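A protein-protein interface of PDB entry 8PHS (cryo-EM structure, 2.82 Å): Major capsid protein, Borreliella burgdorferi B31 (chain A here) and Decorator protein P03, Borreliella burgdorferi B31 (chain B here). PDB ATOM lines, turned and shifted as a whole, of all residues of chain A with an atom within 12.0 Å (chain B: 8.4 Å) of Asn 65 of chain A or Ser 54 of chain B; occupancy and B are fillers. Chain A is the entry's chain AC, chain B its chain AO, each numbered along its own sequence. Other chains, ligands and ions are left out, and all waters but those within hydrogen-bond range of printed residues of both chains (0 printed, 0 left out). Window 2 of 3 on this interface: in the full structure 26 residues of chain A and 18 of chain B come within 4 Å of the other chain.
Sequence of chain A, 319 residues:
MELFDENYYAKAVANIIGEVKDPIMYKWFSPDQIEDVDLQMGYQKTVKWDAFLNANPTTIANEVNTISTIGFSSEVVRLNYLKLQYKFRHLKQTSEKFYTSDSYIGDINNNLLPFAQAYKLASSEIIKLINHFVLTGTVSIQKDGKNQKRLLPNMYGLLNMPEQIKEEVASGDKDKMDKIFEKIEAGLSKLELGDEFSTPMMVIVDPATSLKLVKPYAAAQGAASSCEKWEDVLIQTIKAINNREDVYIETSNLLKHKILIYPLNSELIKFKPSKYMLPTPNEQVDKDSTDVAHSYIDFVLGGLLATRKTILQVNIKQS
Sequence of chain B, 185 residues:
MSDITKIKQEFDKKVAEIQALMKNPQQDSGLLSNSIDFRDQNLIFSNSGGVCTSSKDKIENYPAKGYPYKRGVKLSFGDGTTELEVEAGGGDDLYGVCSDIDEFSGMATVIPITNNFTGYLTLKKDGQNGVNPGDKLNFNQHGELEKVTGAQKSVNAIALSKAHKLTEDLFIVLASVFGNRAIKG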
ATOM      1  N   ASN A  54       9.946 -22.170  32.182  1.00  0.00           N
ATOM      2  CA  ASN A  54      11.231 -21.661  31.724  1.00  0.00           C
ATOM      3  C   ASN A  54      11.481 -20.210  32.110  1.00  0.00           C
ATOM      4  O   ASN A  54      12.641 -19.784  32.125  1.00  0.00           O
ATOM      5  CB  ASN A  54      11.347 -21.803  30.204  1.00  0.00           C
ATOM      6  CG  ASN A  54      11.670 -23.217  29.776  1.00  0.00           C
ATOM      7  OD1 ASN A  54      12.666 -23.795  30.208  1.00  0.00           O
ATOM      8  ND2 ASN A  54      10.830 -23.783  28.920  1.00  0.00           N
ATOM      9  N   ALA A  55      10.438 -19.448  32.424  1.00  0.00           N
ATOM     10  CA  ALA A  55      10.591 -18.040  32.765  1.00  0.00           C
ATOM     11  C   ALA A  55       9.316 -17.567  33.453  1.00  0.00           C
ATOM     12  O   ALA A  55       8.348 -18.316  33.597  1.00  0.00           O
ATOM     13  CB  ALA A  55      10.899 -17.199  31.523  1.00  0.00           C
ATOM     14  N   ASN A  56       9.331 -16.309  33.886  1.00  0.00           N
ATOM     15  CA  ASN A  56       8.141 -15.706  34.460  1.00  0.00           C
ATOM     16  C   ASN A  56       7.064 -15.552  33.386  1.00  0.00           C
ATOM     17  O   ASN A  56       7.375 -15.415  32.202  1.00  0.00           O
ATOM     18  CB  ASN A  56       8.469 -14.343  35.065  1.00  0.00           C
ATOM     19  CG  ASN A  56       9.290 -14.451  36.333  1.00  0.00           C
ATOM     20  OD1 ASN A  56       8.935 -15.179  37.258  1.00  0.00           O
ATOM     21  ND2 ASN A  56      10.395 -13.717  36.384  1.00  0.00           N
ATOM     22  N   PRO A  57       5.790 -15.576  33.775  1.00  0.00           N
ATOM     23  CA  PRO A  57       4.717 -15.449  32.782  1.00  0.00           C
ATOM     24  C   PRO A  57       4.736 -14.088  32.105  1.00  0.00           C
ATOM     25  O   PRO A  57       5.339 -13.127  32.586  1.00  0.00           O
ATOM     26  CB  PRO A  57       3.440 -15.645  33.609  1.00  0.00           C
ATOM     27  CG  PRO A  57       3.839 -15.338  35.009  1.00  0.00           C
ATOM     28  CD  PRO A  57       5.264 -15.771  35.136  1.00  0.00           C
ATOM     29  N   THR A  58       4.075 -14.022  30.954  1.00  0.00           N
ATOM     30  CA  THR A  58       4.041 -12.819  30.131  1.00  0.00           C
ATOM     31  C   THR A  58       2.742 -12.064  30.375  1.00  0.00           C
ATOM     32  O   THR A  58       1.661 -12.660  30.355  1.00  0.00           O
ATOM     33  CB  THR A  58       4.176 -13.176  28.648  1.00  0.00           C
ATOM     34  OG1 THR A  58       5.406 -13.878  28.434  1.00  0.00           O
ATOM     35  CG2 THR A  58       4.167 -11.922  27.794  1.00  0.00           C
ATOM     36  N   THR A  59       2.851 -10.757  30.603  1.00  0.00           N
ATOM     37  CA  THR A  59       1.686  -9.909  30.843  1.00  0.00           C
ATOM     38  C   THR A  59       1.069  -9.519  29.505  1.00  0.00           C
ATOM     39  O   THR A  59       1.675  -8.776  28.729  1.00  0.00           O
ATOM     40  CB  THR A  59       2.082  -8.668  31.638  1.00  0.00           C
ATOM     41  OG1 THR A  59       2.511  -9.053  32.950  1.00  0.00           O
ATOM     42  CG2 THR A  59       0.904  -7.716  31.757  1.00  0.00           C
ATOM     43  N   ILE A  60      -0.146  -9.996  29.238  1.00  0.00           N
ATOM     44  CA  ILE A  60      -0.794  -9.774  27.946  1.00  0.00           C
ATOM     45  C   ILE A  60      -1.452  -8.398  27.974  1.00  0.00           C
ATOM     46  O   ILE A  60      -2.560  -8.233  28.483  1.00  0.00           O
ATOM     47  CB  ILE A  60      -1.803 -10.874  27.615  1.00  0.00           C
ATOM     48  CG1 ILE A  60      -1.107 -12.231  27.600  1.00  0.00           C
ATOM     49  CG2 ILE A  60      -2.461 -10.603  26.272  1.00  0.00           C
ATOM     50  CD1 ILE A  60       0.106 -12.279  26.697  1.00  0.00           C
ATOM     51  N   ALA A  61      -0.762  -7.403  27.421  1.00  0.00           N
ATOM     52  CA  ALA A  61      -1.316  -6.074  27.218  1.00  0.00           C
ATOM     53  C   ALA A  61      -0.794  -5.537  25.895  1.00  0.00           C
ATOM     54  O   ALA A  61       0.383  -5.717  25.571  1.00  0.00           O
ATOM     55  CB  ALA A  61      -0.949  -5.125  28.365  1.00  0.00           C
ATOM     56  N   ASN A  62      -1.671  -4.888  25.138  1.00  0.00           N
ATOM     57  CA  ASN A  62      -1.346  -4.351  23.805  1.00  0.00           C
ATOM     58  C   ASN A  62      -0.879  -5.524  22.934  1.00  0.00           C
ATOM     59  O   ASN A  62      -1.433  -6.629  23.041  1.00  0.00           O
ATOM     60  CB  ASN A  62      -0.359  -3.208  23.926  1.00  0.00           C
ATOM     61  CG  ASN A  62      -0.948  -2.004  24.632  1.00  0.00           C
ATOM     62  OD1 ASN A  62      -2.102  -2.024  25.055  1.00  0.00           O
ATOM     63  ND2 ASN A  62      -0.156  -0.947  24.759  1.00  0.00           N
ATOM     64  N   GLU A  63       0.121  -5.330  22.081  1.00  0.00           N
ATOM     65  CA  GLU A  63       0.557  -6.339  21.123  1.00  0.00           C
ATOM     66  C   GLU A  63       1.884  -6.941  21.563  1.00  0.00           C
ATOM     67  O   GLU A  63       2.808  -6.213  21.939  1.00  0.00           O
ATOM     68  CB  GLU A  63       0.701  -5.736  19.724  1.00  0.00           C
ATOM     69  CG  GLU A  63      -0.546  -5.042  19.213  1.00  0.00           C
ATOM     70  CD  GLU A  63      -0.293  -4.268  17.938  1.00  0.00           C
ATOM     71  OE1 GLU A  63       0.214  -4.869  16.967  1.00  0.00           O
ATOM     72  OE2 GLU A  63      -0.602  -3.058  17.903  1.00  0.00           O
ATOM     73  N   VAL A  64       1.973  -8.267  21.510  1.00  0.00           N
ATOM     74  CA  VAL A  64       3.211  -8.977  21.808  1.00  0.00           C
ATOM     75  C   VAL A  64       3.102 -10.376  21.220  1.00  0.00           C
ATOM     76  O   VAL A  64       2.041 -11.005  21.270  1.00  0.00           O
ATOM     77  CB  VAL A  64       3.494  -9.012  23.331  1.00  0.00           C
ATOM     78  CG1 VAL A  64       2.352  -9.688  24.074  1.00  0.00           C
ATOM     79  CG2 VAL A  64       4.817  -9.708  23.617  1.00  0.00           C
ATOM     80  N   ASN A  65       4.203 -10.853  20.643  1.00  0.00           N
ATOM     81  CA  ASN A  65       4.268 -12.208  20.123  1.00  0.00           C
ATOM     82  C   ASN A  65       5.409 -13.019  20.718  1.00  0.00           C
ATOM     83  O   ASN A  65       5.533 -14.205  20.398  1.00  0.00           O
ATOM     84  CB  ASN A  65       4.396 -12.196  18.592  1.00  0.00           C
ATOM     85  CG  ASN A  65       5.355 -11.138  18.095  1.00  0.00           C
ATOM     86  OD1 ASN A  65       6.510 -11.083  18.514  1.00  0.00           O
ATOM     87  ND2 ASN A  65       4.882 -10.292  17.190  1.00  0.00           N
ATOM     88  N   THR A  66       6.231 -12.425  21.578  1.00  0.00           N
ATOM     89  CA  THR A  66       7.349 -13.111  22.214  1.00  0.00           C
ATOM     90  C   THR A  66       6.932 -13.446  23.643  1.00  0.00           C
ATOM     91  O   THR A  66       6.844 -12.556  24.495  1.00  0.00           O
ATOM     92  CB  THR A  66       8.602 -12.239  22.188  1.00  0.00           C
ATOM     93  OG1 THR A  66       8.945 -11.943  20.830  1.00  0.00           O
ATOM     94  CG2 THR A  66       9.765 -12.964  22.825  1.00  0.00           C
ATOM     95  N   ILE A  67       6.680 -14.726  23.904  1.00  0.00           N
ATOM     96  CA  ILE A  67       6.010 -15.168  25.119  1.00  0.00           C
ATOM     97  C   ILE A  67       6.846 -16.247  25.793  1.00  0.00           C
ATOM     98  O   ILE A  67       7.458 -17.083  25.120  1.00  0.00           O
ATOM     99  CB  ILE A  67       4.590 -15.688  24.809  1.00  0.00           C
ATOM    100  CG1 ILE A  67       3.768 -14.587  24.142  1.00  0.00           C
ATOM    101  CG2 ILE A  67       3.893 -16.172  26.068  1.00  0.00           C
ATOM    102  CD1 ILE A  67       2.415 -15.032  23.699  1.00  0.00           C
ATOM    103  N   SER A  68       6.877 -16.219  27.125  1.00  0.00           N
ATOM    104  CA  SER A  68       7.594 -17.231  27.888  1.00  0.00           C
ATOM    105  C   SER A  68       6.989 -18.608  27.642  1.00  0.00           C
ATOM    106  O   SER A  68       5.786 -18.753  27.409  1.00  0.00           O
ATOM    107  CB  SER A  68       7.557 -16.901  29.378  1.00  0.00           C
ATOM    108  OG  SER A  68       8.246 -15.694  29.649  1.00  0.00           O
ATOM    109  N   THR A  69       7.839 -19.627  27.701  1.00  0.00           N
ATOM    110  CA  THR A  69       7.467 -20.977  27.315  1.00  0.00           C
ATOM    111  C   THR A  69       7.495 -21.913  28.515  1.00  0.00           C
ATOM    112  O   THR A  69       8.092 -21.618  29.554  1.00  0.00           O
ATOM    113  CB  THR A  69       8.399 -21.515  26.223  1.00  0.00           C
ATOM    114  OG1 THR A  69       9.758 -21.409  26.662  1.00  0.00           O
ATOM    115  CG2 THR A  69       8.226 -20.721  24.941  1.00  0.00           C
ATOM    116  N   ILE A  70       6.824 -23.051  28.354  1.00  0.00           N
ATOM    117  CA  ILE A  70       6.822 -24.132  29.330  1.00  0.00           C
ATOM    118  C   ILE A  70       7.464 -25.347  28.680  1.00  0.00           C
ATOM    119  O   ILE A  70       7.033 -25.781  27.605  1.00  0.00           O
ATOM    120  CB  ILE A  70       5.399 -24.461  29.816  1.00  0.00           C
ATOM    121  CG1 ILE A  70       4.861 -23.339  30.703  1.00  0.00           C
ATOM    122  CG2 ILE A  70       5.374 -25.789  30.551  1.00  0.00           C
ATOM    123  CD1 ILE A  70       3.455 -23.579  31.193  1.00  0.00           C
ATOM    124  N   GLY B  50      14.299 -21.877  23.008  1.00  0.00           N
ATOM    125  CA  GLY B  50      14.466 -20.681  23.800  1.00  0.00           C
ATOM    126  C   GLY B  50      13.540 -20.653  25.002  1.00  0.00           C
ATOM    127  O   GLY B  50      12.574 -21.407  25.086  1.00  0.00           O
ATOM    128  N   VAL B  51      13.854 -19.765  25.946  1.00  0.00           N
ATOM    129  CA  VAL B  51      13.015 -19.618  27.131  1.00  0.00           C
ATOM    130  C   VAL B  51      11.792 -18.761  26.825  1.00  0.00           C
ATOM    131  O   VAL B  51      10.686 -19.050  27.295  1.00  0.00           O
ATOM    132  CB  VAL B  51      13.837 -19.050  28.303  1.00  0.00           C
ATOM    133  CG1 VAL B  51      14.870 -20.065  28.759  1.00  0.00           C
ATOM    134  CG2 VAL B  51      14.521 -17.751  27.905  1.00  0.00           C
ATOM    135  N   CYS B  52      11.967 -17.703  26.037  1.00  0.00           N
ATOM    136  CA  CYS B  52      10.878 -16.823  25.626  1.00  0.00           C
ATOM    137  C   CYS B  52      10.958 -16.696  24.111  1.00  0.00           C
ATOM    138  O   CYS B  52      11.853 -16.022  23.590  1.00  0.00           O
ATOM    139  CB  CYS B  52      10.988 -15.461  26.312  1.00  0.00           C
ATOM    140  SG  CYS B  52       9.591 -14.345  26.060  1.00  0.00           S
ATOM    141  N   THR B  53      10.031 -17.340  23.407  1.00  0.00           N
ATOM    142  CA  THR B  53      10.108 -17.491  21.961  1.00  0.00           C
ATOM    143  C   THR B  53       8.948 -16.778  21.282  1.00  0.00           C
ATOM    144  O   THR B  53       7.841 -16.694  21.823  1.00  0.00           O
ATOM    145  CB  THR B  53      10.108 -18.975  21.560  1.00  0.00           C
ATOM    146  OG1 THR B  53      10.999 -19.703  22.413  1.00  0.00           O
ATOM    147  CG2 THR B  53      10.557 -19.145  20.116  1.00  0.00           C
ATOM    148  N   SER B  54       9.215 -16.265  20.084  1.00  0.00           N
ATOM    149  CA  SER B  54       8.215 -15.609  19.258  1.00  0.00           C
ATOM    150  C   SER B  54       7.746 -16.545  18.154  1.00  0.00           C
ATOM    151  O   SER B  54       8.512 -17.360  17.636  1.00  0.00           O
ATOM    152  CB  SER B  54       8.776 -14.325  18.645  1.00  0.00           C
ATOM    153  OG  SER B  54       7.890 -13.789  17.680  1.00  0.00           O
ATOM    154  N   SER B  55       6.465 -16.423  17.800  1.00  0.00           N
ATOM    155  CA  SER B  55       5.917 -17.205  16.701  1.00  0.00           C
ATOM    156  C   SER B  55       6.420 -16.741  15.342  1.00  0.00           C
ATOM    157  O   SER B  55       6.270 -17.476  14.361  1.00  0.00           O
ATOM    158  CB  SER B  55       4.389 -17.152  16.730  1.00  0.00           C
ATOM    159  OG  SER B  55       3.925 -15.814  16.686  1.00  0.00           O
ATOM    160  N   LYS B  56       7.011 -15.550  15.261  1.00  0.00           N
ATOM    161  CA  LYS B  56       7.522 -14.997  14.014  1.00  0.00           C
ATOM    162  C   LYS B  56       9.026 -15.193  13.867  1.00  0.00           C
ATOM    163  O   LYS B  56       9.707 -14.351  13.270  1.00  0.00           O
ATOM    164  CB  LYS B  56       7.168 -13.514  13.914  1.00  0.00           C
ATOM    165  CG  LYS B  56       5.714 -13.194  14.214  1.00  0.00           C
ATOM    166  CD  LYS B  56       4.779 -13.931  13.272  1.00  0.00           C
ATOM    167  CE  LYS B  56       3.341 -13.863  13.755  1.00  0.00           C
ATOM    168  NZ  LYS B  56       2.915 -12.460  14.011  1.00  0.00           N
ATOM    169  N   ASP B  57       9.561 -16.288  14.398  1.00  0.00           N
ATOM    170  CA  ASP B  57      10.993 -16.553  14.373  1.00  0.00           C
ATOM    171  C   ASP B  57      11.335 -17.444  13.188  1.00  0.00           C
ATOM    172  O   ASP B  57      10.692 -18.476  12.973  1.00  0.00           O
ATOM    173  CB  ASP B  57      11.448 -17.212  15.675  1.00  0.00           C
ATOM    174  CG  ASP B  57      11.721 -16.204  16.773  1.00  0.00           C
ATOM    175  OD1 ASP B  57      12.313 -15.146  16.475  1.00  0.00           O
ATOM    176  OD2 ASP B  57      11.351 -16.473  17.935  1.00  0.00           O
ATOM    177  N   LYS B  58      12.350 -17.043  12.425  1.00  0.00           N
ATOM    178  CA  LYS B  58      12.810 -17.831  11.291  1.00  0.00           C
ATOM    179  C   LYS B  58      13.753 -18.926  11.773  1.00  0.00           C
ATOM    180  O   LYS B  58      14.736 -18.650  12.467  1.00  0.00           O
ATOM    181  CB  LYS B  58      13.509 -16.937  10.269  1.00  0.00           C
ATOM    182  CG  LYS B  58      14.021 -17.681   9.049  1.00  0.00           C
ATOM    183  CD  LYS B  58      14.655 -16.730   8.052  1.00  0.00           C
ATOM    184  CE  LYS B  58      15.095 -17.462   6.798  1.00  0.00           C
ATOM    185  NZ  LYS B  58      15.725 -16.543   5.812  1.00  0.00           N
ATOM    186  N   ILE B  59      13.449 -20.167  11.405  1.00  0.00           N
ATOM    187  CA  ILE B  59      14.168 -21.339  11.890  1.00  0.00           C
ATOM    188  C   ILE B  59      14.613 -22.167  10.693  1.00  0.00           C
ATOM    189  O   ILE B  59      13.776 -22.588   9.884  1.00  0.00           O
ATOM    190  CB  ILE B  59      13.301 -22.186  12.835  1.00  0.00           C
ATOM    191  CG1 ILE B  59      12.819 -21.345  14.019  1.00  0.00           C
ATOM    192  CG2 ILE B  59      14.060 -23.405  13.299  1.00  0.00           C
ATOM    193  CD1 ILE B  59      11.842 -22.063  14.918  1.00  0.00           C
ATOM    194  N   ASN B 115      18.288 -13.142  13.433  1.00  0.00           N
ATOM    195  CA  ASN B 115      17.099 -13.285  14.263  1.00  0.00           C
ATOM    196  C   ASN B 115      17.540 -13.401  15.716  1.00  0.00           C
ATOM    197  O   ASN B 115      18.326 -14.291  16.059  1.00  0.00           O
ATOM    198  CB  ASN B 115      16.284 -14.507  13.842  1.00  0.00           C
ATOM    199  CG  ASN B 115      14.886 -14.502  14.420  1.00  0.00           C
ATOM    200  OD1 ASN B 115      14.290 -13.445  14.622  1.00  0.00           O
ATOM    201  ND2 ASN B 115      14.351 -15.687  14.687  1.00  0.00           N
ATOM    202  N   ASN B 116      17.037 -12.507  16.563  1.00  0.00           N
ATOM    203  CA  ASN B 116      17.458 -12.476  17.955  1.00  0.00           C
ATOM    204  C   ASN B 116      16.979 -13.719  18.698  1.00  0.00           C
ATOM    205  O   ASN B 116      15.944 -14.307  18.375  1.00  0.00           O
ATOM    206  CB  ASN B 116      16.938 -11.214  18.642  1.00  0.00           C
ATOM    207  CG  ASN B 116      15.441 -11.237  18.850  1.00  0.00           C
ATOM    208  OD1 ASN B 116      14.676 -11.399  17.902  1.00  0.00           O
ATOM    209  ND2 ASN B 116      15.013 -11.070  20.096  1.00  0.00           N
ATOM    210  N   PHE B 117      17.755 -14.117  19.704  1.00  0.00           N
ATOM    211  CA  PHE B 117      17.504 -15.339  20.453  1.00  0.00           C
ATOM    212  C   PHE B 117      17.790 -15.094  21.927  1.00  0.00           C
ATOM    213  O   PHE B 117      18.671 -14.308  22.280  1.00  0.00           O
ATOM    214  CB  PHE B 117      18.365 -16.497  19.927  1.00  0.00           C
ATOM    215  CG  PHE B 117      18.327 -17.727  20.785  1.00  0.00           C
ATOM    216  CD1 PHE B 117      17.199 -18.529  20.822  1.00  0.00           C
ATOM    217  CD2 PHE B 117      19.419 -18.084  21.557  1.00  0.00           C
ATOM    218  CE1 PHE B 117      17.163 -19.663  21.610  1.00  0.00           C
ATOM    219  CE2 PHE B 117      19.388 -19.215  22.346  1.00  0.00           C
ATOM    220  CZ  PHE B 117      18.257 -20.006  22.373  1.00  0.00           C
ATOM    221  N   THR B 118      17.031 -15.775  22.784  1.00  0.00           N
ATOM    222  CA  THR B 118      17.211 -15.693  24.228  1.00  0.00           C
ATOM    223  C   THR B 118      17.032 -17.085  24.811  1.00  0.00           C
ATOM    224  O   THR B 118      15.951 -17.668  24.697  1.00  0.00           O
ATOM    225  CB  THR B 118      16.217 -14.717  24.862  1.00  0.00           C
ATOM    226  OG1 THR B 118      16.352 -13.428  24.250  1.00  0.00           O
ATOM    227  CG2 THR B 118      16.475 -14.590  26.354  1.00  0.00           C
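OG1 of Thr 69 of chain A sits at hydrogen-bond distance from O of Val 51 of chain B (2.6 Å).
The side-chain hydroxyl (OG) of Ser 54 of chain B sits at hydrogen-bond distance from the side-chain amide oxygen (OD1) of Asn 65 of chain A (3.1 Å).
The backbone carbonyl oxygen of Thr 53 of chain B sits at hydrogen-bond distance from the backbone NH of Ile 67 of chain A, 3.1 Å away.
SG of Cys 52 of chain B sits at hydrogen-bond distance from N of Ser 68 of chain A, 3.5 Å away.
The backbone carbonyl oxygen of Thr 66 of chain A sits close to the side-chain sulfur of Cys 52 of chain B.
The backbone carbonyl oxygen (O) of Ile 67 of chain A lies close to the side-chain sulfur (SG) of Cys 52 of chain B, 3.6 Å away.
The side-chain hydroxyl (OG1) of Thr 69 of chain A sits at hydrogen-bond distance from the backbone carbonyl oxygen (O) of Gly 50 of chain B, 3.2 Å away.
N of Val 51 of chain B is in hydrogen-bond range of O of Thr 118 of chain B.
The backbone NH of Asn 54 of chain A is in hydrogen-bond range of the backbone carbonyl oxygen of Thr 69 of chain A.
The side-chain carboxylate (OD2) of Asp 57 of chain B sits at hydrogen-bond distance from the backbone NH (N) of Ser 54 of chain B, at 3.0 Å.
OG of Ser 68 of chain A is in hydrogen-bond range of O of Asn 56 of chain A (2.7 Å).
N of Lys 56 of chain B sits at hydrogen-bond distance from OG of Ser 54 of chain B (3.1 Å).
The side-chain amide oxygen (OD1) of Asn 65 of chain A lies within hydrogen-bond range of the side-chain hydroxyl (OG1) of Thr 66 of chain A, at 3.5 Å.
No residue of chain B comes within 4 Å of Val 64 of chain A.
Asn 65 of chain A touches just these residues of chain B: Thr 53, Ser 54 and Ser 55.
Thr 66 of chain A touches just these residues of chain B: Cys 52, Thr 53 and Ser 54.
Printed residues of chain B within 4 Å of Ile 67 of chain A: Cys 52 (3.4 Å) and Thr 53 (3.1 Å).
Of the printed residues of chain B, Ser 68 of chain A touches Val 51 and Cys 52.
Printed residues of chain B within 4 Å of Thr 69 of chain A: Gly 50 (3.2 Å), Val 51 (2.6 Å) and Thr 53 (3.9 Å).
Of the printed residues of chain A, Gly 50 of chain B touches Thr 69.
Of the printed residues of chain A, Val 51 of chain B touches Ser 68 (3.6 Å) and Thr 69 (2.6 Å).
Of chain A, only Thr 66 (3.5 Å), Ile 67 (3.4 Å) and Ser 68 (3.5 Å) come within 4 Å of Cys 52 of chain B.
Printed residues of chain A within 4 Å of Thr 53 of chain B: Asn 65 (3.7 Å), Thr 66 (3.6 Å), Ile 67 (3.1 Å) and Thr 69 (3.9 Å).
Ser 54 of chain B touches just these residues of chain A: Asn 65 (3.1 Å) and Thr 66 (3.2 Å).
No residue of chain A comes within 4 Å of Lys 56 of chain B.
The nearest printed residue of chain A that does not touch Val 51 of chain B is Asn 54 of chain A (4.05 Å).
Printed residues of chain A that touch a printed residue of chain B: Asn 65, Thr 66, Ile 67, Ser 68 and Thr 69.
Thr 53 of chain B touches Asn 65 of chain A (O to O, 3.7 Å).
O of Asn 65 of chain A touches N of Ser 55 of chain B, at 3.5 Å.
Thr 53 of chain B touches Thr 66 of chain A (O to CA, 3.6 Å).
Ser 54 of chain B touches Thr 66 of chain A.
Ser 68 of chain A touches Val 51 of chain B.
Thr 69 of chain A touches Thr 53 of chain B (CG2 to OG1, 3.9 Å).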
